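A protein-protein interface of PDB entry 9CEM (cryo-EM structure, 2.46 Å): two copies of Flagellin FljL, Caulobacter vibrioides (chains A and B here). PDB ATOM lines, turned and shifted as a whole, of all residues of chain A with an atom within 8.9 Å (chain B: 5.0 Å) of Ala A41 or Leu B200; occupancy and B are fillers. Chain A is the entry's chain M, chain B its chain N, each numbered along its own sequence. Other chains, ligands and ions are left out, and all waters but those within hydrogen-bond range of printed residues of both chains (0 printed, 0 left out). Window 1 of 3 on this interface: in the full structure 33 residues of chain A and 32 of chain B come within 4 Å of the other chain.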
ATOM      1  N   LYS A  37      13.275 -23.937  13.907  1.00  0.00           N
ATOM      2  CA  LYS A  37      14.131 -25.048  13.508  1.00  0.00           C
ATOM      3  C   LYS A  37      13.583 -25.808  12.309  1.00  0.00           C
ATOM      4  O   LYS A  37      14.298 -26.639  11.739  1.00  0.00           O
ATOM      5  CB  LYS A  37      14.337 -26.007  14.683  1.00  0.00           C
ATOM      6  CG  LYS A  37      13.078 -26.699  15.165  1.00  0.00           C
ATOM      7  CD  LYS A  37      13.379 -27.579  16.366  1.00  0.00           C
ATOM      8  CE  LYS A  37      12.138 -28.306  16.858  1.00  0.00           C
ATOM      9  NZ  LYS A  37      11.126 -27.377  17.432  1.00  0.00           N
ATOM     10  N   VAL A  38      12.341 -25.546  11.918  1.00  0.00           N
ATOM     11  CA  VAL A  38      11.730 -26.147  10.732  1.00  0.00           C
ATOM     12  C   VAL A  38      11.043 -25.002   9.993  1.00  0.00           C
ATOM     13  O   VAL A  38       9.813 -24.896   9.962  1.00  0.00           O
ATOM     14  CB  VAL A  38      10.750 -27.271  11.081  1.00  0.00           C
ATOM     15  CG1 VAL A  38      10.165 -27.899   9.817  1.00  0.00           C
ATOM     16  CG2 VAL A  38      11.420 -28.332  11.942  1.00  0.00           C
ATOM     17  N   ALA A  39      11.842 -24.107   9.410  1.00  0.00           N
ATOM     18  CA  ALA A  39      11.321 -22.919   8.752  1.00  0.00           C
ATOM     19  C   ALA A  39      10.789 -23.172   7.348  1.00  0.00           C
ATOM     20  O   ALA A  39      10.118 -22.293   6.795  1.00  0.00           O
ATOM     21  CB  ALA A  39      12.401 -21.828   8.689  1.00  0.00           C
ATOM     22  N   ASN A  40      11.054 -24.338   6.764  1.00  0.00           N
ATOM     23  CA  ASN A  40      10.637 -24.622   5.395  1.00  0.00           C
ATOM     24  C   ASN A  40      10.595 -26.132   5.198  1.00  0.00           C
ATOM     25  O   ASN A  40      10.974 -26.905   6.081  1.00  0.00           O
ATOM     26  CB  ASN A  40      11.569 -23.966   4.375  1.00  0.00           C
ATOM     27  CG  ASN A  40      13.030 -24.213   4.681  1.00  0.00           C
ATOM     28  OD1 ASN A  40      13.497 -25.350   4.641  1.00  0.00           O
ATOM     29  ND2 ASN A  40      13.759 -23.150   4.993  1.00  0.00           N
ATOM     30  N   ALA A  41      10.104 -26.541   4.024  1.00  0.00           N
ATOM     31  CA  ALA A  41      10.025 -27.959   3.688  1.00  0.00           C
ATOM     32  C   ALA A  41      11.392 -28.622   3.619  1.00  0.00           C
ATOM     33  O   ALA A  41      11.504 -29.819   3.912  1.00  0.00           O
ATOM     34  CB  ALA A  41       9.304 -28.143   2.354  1.00  0.00           C
ATOM     35  N   LYS A  42      12.433 -27.880   3.238  1.00  0.00           N
ATOM     36  CA  LYS A  42      13.759 -28.465   3.094  1.00  0.00           C
ATOM     37  C   LYS A  42      14.320 -28.956   4.422  1.00  0.00           C
ATOM     38  O   LYS A  42      15.075 -29.935   4.446  1.00  0.00           O
ATOM     39  CB  LYS A  42      14.716 -27.443   2.477  1.00  0.00           C
ATOM     40  CG  LYS A  42      16.097 -27.995   2.162  1.00  0.00           C
ATOM     41  CD  LYS A  42      17.034 -26.925   1.619  1.00  0.00           C
ATOM     42  CE  LYS A  42      16.706 -26.528   0.191  1.00  0.00           C
ATOM     43  NZ  LYS A  42      17.717 -25.568  -0.343  1.00  0.00           N
ATOM     44  N   ASP A  43      13.964 -28.302   5.529  1.00  0.00           N
ATOM     45  CA  ASP A  43      14.503 -28.703   6.824  1.00  0.00           C
ATOM     46  C   ASP A  43      13.957 -30.056   7.263  1.00  0.00           C
ATOM     47  O   ASP A  43      14.702 -30.890   7.790  1.00  0.00           O
ATOM     48  CB  ASP A  43      14.192 -27.630   7.867  1.00  0.00           C
ATOM     49  CG  ASP A  43      14.816 -26.289   7.526  1.00  0.00           C
ATOM     50  OD1 ASP A  43      15.906 -26.274   6.917  1.00  0.00           O
ATOM     51  OD2 ASP A  43      14.211 -25.249   7.859  1.00  0.00           O
ATOM     52  N   ASN A  44      12.666 -30.299   7.035  1.00  0.00           N
ATOM     53  CA  ASN A  44      12.014 -31.532   7.458  1.00  0.00           C
ATOM     54  C   ASN A  44      10.599 -31.567   6.898  1.00  0.00           C
ATOM     55  O   ASN A  44       9.716 -30.864   7.396  1.00  0.00           O
ATOM     56  CB  ASN A  44      11.995 -31.635   8.986  1.00  0.00           C
ATOM     57  CG  ASN A  44      11.597 -33.012   9.478  1.00  0.00           C
ATOM     58  OD1 ASN A  44      10.921 -33.767   8.781  1.00  0.00           O
ATOM     59  ND2 ASN A  44      12.024 -33.349  10.688  1.00  0.00           N
ATOM     60  N   GLY A  45      10.369 -32.391   5.874  1.00  0.00           N
ATOM     61  CA  GLY A  45       9.109 -32.326   5.152  1.00  0.00           C
ATOM     62  C   GLY A  45       7.904 -32.759   5.964  1.00  0.00           C
ATOM     63  O   GLY A  45       6.819 -32.192   5.816  1.00  0.00           O
ATOM     64  N   ALA A  46       8.072 -33.754   6.835  1.00  0.00           N
ATOM     65  CA  ALA A  46       6.929 -34.277   7.578  1.00  0.00           C
ATOM     66  C   ALA A  46       6.430 -33.273   8.611  1.00  0.00           C
ATOM     67  O   ALA A  46       5.233 -32.951   8.659  1.00  0.00           O
ATOM     68  CB  ALA A  46       7.310 -35.595   8.251  1.00  0.00           C
ATOM     69  N   ILE A  47       7.338 -32.762   9.445  1.00  0.00           N
ATOM     70  CA  ILE A  47       6.950 -31.778  10.447  1.00  0.00           C
ATOM     71  C   ILE A  47       6.476 -30.500   9.774  1.00  0.00           C
ATOM     72  O   ILE A  47       5.546 -29.838  10.258  1.00  0.00           O
ATOM     73  CB  ILE A  47       8.127 -31.529  11.410  1.00  0.00           C
ATOM     74  CG1 ILE A  47       8.221 -32.660  12.435  1.00  0.00           C
ATOM     75  CG2 ILE A  47       7.981 -30.197  12.129  1.00  0.00           C
ATOM     76  CD1 ILE A  47       9.587 -32.796  13.067  1.00  0.00           C
ATOM     77  N   TRP A  48       7.062 -30.162   8.622  1.00  0.00           N
ATOM     78  CA  TRP A  48       6.633 -28.971   7.899  1.00  0.00           C
ATOM     79  C   TRP A  48       5.204 -29.119   7.400  1.00  0.00           C
ATOM     80  O   TRP A  48       4.394 -28.200   7.546  1.00  0.00           O
ATOM     81  CB  TRP A  48       7.570 -28.704   6.723  1.00  0.00           C
ATOM     82  CG  TRP A  48       7.235 -27.463   5.960  1.00  0.00           C
ATOM     83  CD1 TRP A  48       7.417 -26.176   6.371  1.00  0.00           C
ATOM     84  CD2 TRP A  48       6.617 -27.389   4.671  1.00  0.00           C
ATOM     85  NE1 TRP A  48       6.978 -25.304   5.405  1.00  0.00           N
ATOM     86  CE2 TRP A  48       6.477 -26.024   4.353  1.00  0.00           C
ATOM     87  CE3 TRP A  48       6.174 -28.344   3.751  1.00  0.00           C
ATOM     88  CZ2 TRP A  48       5.916 -25.591   3.156  1.00  0.00           C
ATOM     89  CZ3 TRP A  48       5.620 -27.912   2.563  1.00  0.00           C
ATOM     90  CH2 TRP A  48       5.495 -26.548   2.275  1.00  0.00           C
ATOM     91  N   SER A  49       4.873 -30.273   6.811  1.00  0.00           N
ATOM     92  CA  SER A  49       3.517 -30.481   6.316  1.00  0.00           C
ATOM     93  C   SER A  49       2.509 -30.515   7.457  1.00  0.00           C
ATOM     94  O   SER A  49       1.399 -29.981   7.328  1.00  0.00           O
ATOM     95  CB  SER A  49       3.451 -31.774   5.503  1.00  0.00           C
ATOM     96  OG  SER A  49       4.260 -31.691   4.345  1.00  0.00           O
ATOM     97  N   LYS A  52       2.055 -26.971   8.649  1.00  0.00           N
ATOM     98  CA  LYS A  52       1.381 -26.174   7.634  1.00  0.00           C
ATOM     99  C   LYS A  52      -0.115 -26.453   7.616  1.00  0.00           C
ATOM    100  O   LYS A  52      -0.932 -25.519   7.600  1.00  0.00           O
ATOM    101  CB  LYS A  52       1.996 -26.458   6.265  1.00  0.00           C
ATOM    102  CG  LYS A  52       1.393 -25.651   5.142  1.00  0.00           C
ATOM    103  CD  LYS A  52       1.650 -24.178   5.358  1.00  0.00           C
ATOM    104  CE  LYS A  52       3.120 -23.853   5.175  1.00  0.00           C
ATOM    105  NZ  LYS A  52       3.383 -22.398   5.323  1.00  0.00           N
ATOM    106  N   ALA B  78      11.480 -23.526  -7.172  1.00  0.00           N
ATOM    107  CA  ALA B  78      10.198 -24.213  -7.057  1.00  0.00           C
ATOM    108  C   ALA B  78       9.602 -24.038  -5.665  1.00  0.00           C
ATOM    109  O   ALA B  78       8.401 -23.778  -5.525  1.00  0.00           O
ATOM    110  CB  ALA B  78      10.361 -25.695  -7.389  1.00  0.00           C
ATOM    111  N   LEU B  79      10.429 -24.153  -4.623  1.00  0.00           N
ATOM    112  CA  LEU B  79       9.928 -23.917  -3.269  1.00  0.00           C
ATOM    113  C   LEU B  79       9.522 -22.460  -3.061  1.00  0.00           C
ATOM    114  O   LEU B  79       8.526 -22.179  -2.367  1.00  0.00           O
ATOM    115  CB  LEU B  79      10.987 -24.327  -2.245  1.00  0.00           C
ATOM    116  CG  LEU B  79      11.331 -25.817  -2.178  1.00  0.00           C
ATOM    117  CD1 LEU B  79      12.490 -26.070  -1.226  1.00  0.00           C
ATOM    118  CD2 LEU B  79      10.114 -26.629  -1.764  1.00  0.00           C
ATOM    119  N   GLY B  82       6.189 -22.296  -4.380  1.00  0.00           N
ATOM    120  CA  GLY B  82       5.229 -23.166  -3.727  1.00  0.00           C
ATOM    121  C   GLY B  82       4.716 -22.606  -2.416  1.00  0.00           C
ATOM    122  O   GLY B  82       3.557 -22.827  -2.053  1.00  0.00           O
ATOM    123  N   ASP B  83       5.561 -21.877  -1.682  1.00  0.00           N
ATOM    124  CA  ASP B  83       5.045 -21.259  -0.459  1.00  0.00           C
ATOM    125  C   ASP B  83       3.953 -20.238  -0.770  1.00  0.00           C
ATOM    126  O   ASP B  83       2.940 -20.162  -0.055  1.00  0.00           O
ATOM    127  CB  ASP B  83       6.179 -20.604   0.326  1.00  0.00           C
ATOM    128  CG  ASP B  83       6.983 -19.656  -0.521  1.00  0.00           C
ATOM    129  OD1 ASP B  83       6.778 -19.673  -1.750  1.00  0.00           O
ATOM    130  OD2 ASP B  83       7.810 -18.902   0.031  1.00  0.00           O
ATOM    131  N   THR B  86       0.848 -22.022  -1.457  1.00  0.00           N
ATOM    132  CA  THR B  86       0.250 -22.501  -0.216  1.00  0.00           C
ATOM    133  C   THR B  86      -0.575 -21.420   0.473  1.00  0.00           C
ATOM    134  O   THR B  86      -1.715 -21.674   0.884  1.00  0.00           O
ATOM    135  CB  THR B  86       1.339 -23.009   0.727  1.00  0.00           C
ATOM    136  OG1 THR B  86       1.867 -24.245   0.231  1.00  0.00           O
ATOM    137  CG2 THR B  86       0.774 -23.222   2.113  1.00  0.00           C
ATOM    138  N   LEU B 163       2.579 -28.020  -9.655  1.00  0.00           N
ATOM    139  CA  LEU B 163       1.882 -27.125  -8.738  1.00  0.00           C
ATOM    140  C   LEU B 163       0.837 -26.261  -9.432  1.00  0.00           C
ATOM    141  O   LEU B 163       0.270 -25.366  -8.795  1.00  0.00           O
ATOM    142  CB  LEU B 163       2.887 -26.244  -7.993  1.00  0.00           C
ATOM    143  CG  LEU B 163       3.807 -27.018  -7.051  1.00  0.00           C
ATOM    144  CD1 LEU B 163       4.863 -26.106  -6.455  1.00  0.00           C
ATOM    145  CD2 LEU B 163       2.993 -27.690  -5.957  1.00  0.00           C
ATOM    146  N   ALA B 196      -0.544 -30.195  -2.316  1.00  0.00           N
ATOM    147  CA  ALA B 196       0.498 -29.193  -2.529  1.00  0.00           C
ATOM    148  C   ALA B 196       1.599 -29.304  -1.478  1.00  0.00           C
ATOM    149  O   ALA B 196       2.793 -29.284  -1.812  1.00  0.00           O
ATOM    150  CB  ALA B 196      -0.116 -27.794  -2.521  1.00  0.00           C
ATOM    151  N   THR B 197       1.222 -29.425  -0.200  1.00  0.00           N
ATOM    152  CA  THR B 197       2.249 -29.582   0.829  1.00  0.00           C
ATOM    153  C   THR B 197       3.034 -30.877   0.650  1.00  0.00           C
ATOM    154  O   THR B 197       4.250 -30.902   0.891  1.00  0.00           O
ATOM    155  CB  THR B 197       1.630 -29.528   2.226  1.00  0.00           C
ATOM    156  OG1 THR B 197       0.832 -30.698   2.451  1.00  0.00           O
ATOM    157  CG2 THR B 197       0.786 -28.276   2.396  1.00  0.00           C
ATOM    158  N   ASN B 198       2.377 -31.947   0.192  1.00  0.00           N
ATOM    159  CA  ASN B 198       3.107 -33.193  -0.032  1.00  0.00           C
ATOM    160  C   ASN B 198       4.124 -33.046  -1.161  1.00  0.00           C
ATOM    161  O   ASN B 198       5.270 -33.510  -1.045  1.00  0.00           O
ATOM    162  CB  ASN B 198       2.130 -34.330  -0.335  1.00  0.00           C
ATOM    163  CG  ASN B 198       1.232 -34.663   0.844  1.00  0.00           C
ATOM    164  OD1 ASN B 198       1.371 -34.089   1.923  1.00  0.00           O
ATOM    165  ND2 ASN B 198       0.295 -35.580   0.637  1.00  0.00           N
ATOM    166  N   LYS B 199       3.732 -32.386  -2.255  1.00  0.00           N
ATOM    167  CA  LYS B 199       4.671 -32.199  -3.355  1.00  0.00           C
ATOM    168  C   LYS B 199       5.837 -31.304  -2.947  1.00  0.00           C
ATOM    169  O   LYS B 199       6.986 -31.547  -3.344  1.00  0.00           O
ATOM    170  CB  LYS B 199       3.939 -31.632  -4.573  1.00  0.00           C
ATOM    171  CG  LYS B 199       2.952 -32.617  -5.191  1.00  0.00           C
ATOM    172  CD  LYS B 199       2.261 -32.047  -6.415  1.00  0.00           C
ATOM    173  CE  LYS B 199       1.268 -33.037  -7.003  1.00  0.00           C
ATOM    174  NZ  LYS B 199       0.578 -32.483  -8.197  1.00  0.00           N
ATOM    175  N   LEU B 200       5.572 -30.282  -2.126  1.00  0.00           N
ATOM    176  CA  LEU B 200       6.672 -29.438  -1.673  1.00  0.00           C
ATOM    177  C   LEU B 200       7.627 -30.195  -0.758  1.00  0.00           C
ATOM    178  O   LEU B 200       8.848 -29.992  -0.834  1.00  0.00           O
ATOM    179  CB  LEU B 200       6.140 -28.185  -0.977  1.00  0.00           C
ATOM    180  CG  LEU B 200       5.474 -27.174  -1.911  1.00  0.00           C
ATOM    181  CD1 LEU B 200       4.341 -26.439  -1.214  1.00  0.00           C
ATOM    182  CD2 LEU B 200       6.507 -26.207  -2.460  1.00  0.00           C
ATOM    183  N   SER B 201       7.107 -31.082   0.097  1.00  0.00           N
ATOM    184  CA  SER B 201       8.003 -31.881   0.928  1.00  0.00           C
ATOM    185  C   SER B 201       8.851 -32.823   0.079  1.00  0.00           C
ATOM    186  O   SER B 201      10.035 -33.042   0.372  1.00  0.00           O
ATOM    187  CB  SER B 201       7.202 -32.660   1.974  1.00  0.00           C
ATOM    188  OG  SER B 201       6.367 -33.630   1.371  1.00  0.00           O
ATOM    189  N   SER B 202       8.276 -33.362  -1.002  1.00  0.00           N
ATOM    190  CA  SER B 202       9.076 -34.209  -1.886  1.00  0.00           C
ATOM    191  C   SER B 202      10.183 -33.411  -2.569  1.00  0.00           C
ATOM    192  O   SER B 202      11.322 -33.886  -2.692  1.00  0.00           O
ATOM    193  CB  SER B 202       8.183 -34.887  -2.923  1.00  0.00           C
ATOM    194  OG  SER B 202       7.428 -35.930  -2.337  1.00  0.00           O
ATOM    195  N   LEU B 203       9.875 -32.182  -2.996  1.00  0.00           N
ATOM    196  CA  LEU B 203      10.913 -31.358  -3.611  1.00  0.00           C
ATOM    197  C   LEU B 203      12.013 -31.006  -2.614  1.00  0.00           C
ATOM    198  O   LEU B 203      13.201 -30.981  -2.970  1.00  0.00           O
ATOM    199  CB  LEU B 203      10.305 -30.088  -4.202  1.00  0.00           C
ATOM    200  CG  LEU B 203       9.582 -30.224  -5.541  1.00  0.00           C
ATOM    201  CD1 LEU B 203       8.457 -29.211  -5.638  1.00  0.00           C
ATOM    202  CD2 LEU B 203      10.562 -30.052  -6.688  1.00  0.00           C
ATOM    203  N   GLY B 204      11.649 -30.778  -1.350  1.00  0.00           N
ATOM    204  CA  GLY B 204      12.670 -30.464  -0.364  1.00  0.00           C
ATOM    205  C   GLY B 204      13.562 -31.653  -0.060  1.00  0.00           C
ATOM    206  O   GLY B 204      14.779 -31.505   0.119  1.00  0.00           O
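O of Gly A45 sits at hydrogen-bond distance from OG of Ser A49. OG1 of Thr B86 sits at hydrogen-bond distance from O of Gly B82, at 3.2 Å. The side-chain hydroxyl (OG1) of Thr B197 is in hydrogen-bond range of the side-chain amide oxygen (OD1) of Asn B198. O of Thr B197 lies within hydrogen-bond range of OG of Ser B201 (3.5 Å). O of Asn B198 is in hydrogen-bond range of OG of Ser B201 (2.7 Å).
Hydrophobic or aromatic side chains of chain A that line the printed part of chain B: Ala A41 and Trp A48. Among the printed residues, 8 pairs touch across the chains.
Leu B200 touches two residues of chain A. No residue of chain A comes within 4 Å of Gly B82. Ser B201 touches just these residues of chain A: Gly A45 and Ser A49. Printed residues of chain B within 4 Å of Trp A48: Thr B197 (3.7 Å) and Leu B200 (3.6 Å). Of the printed residues of chain B, Lys A52 touches Thr B86 and Thr B197. Of the printed residues of chain A, Thr B86 touches Lys A52. Of the printed residues of chain B, Gly A45 touches Ser B201 (3.7 Å). Printed residues of chain B within 4 Å of Ser A49: Thr B197 and Ser B201. Asn B198 touches none of the printed residues of chain A. Ser B202 touches none of the printed residues of chain A. The nearest residue of chain B that does not touch Ala A41 is Ser B201 (4.2 Å). The nearest residue of chain A that does not touch Leu B200 is Lys A42 (5.8 Å).
No position is printed for both chains. Of the 8 pairs that touch across the chains among the printed residues, none has its exchanged pair printed and touching as well.
Among the printed residues, pairs that only touch across the chains: Lys A52 with Thr B86 (3.5 Å), Ser A49 with Thr B197 (3.5 Å), Trp A48 with Leu B200 (3.6 Å), Trp A48 with Thr B197 (3.7 Å), Ala A41 with Leu B200 (3.7 Å), Gly A45 with Ser B201 (3.7 Å), Lys A52 with Thr B197 (3.8 Å) and Ser A49 with Ser B201 (3.9 Å).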
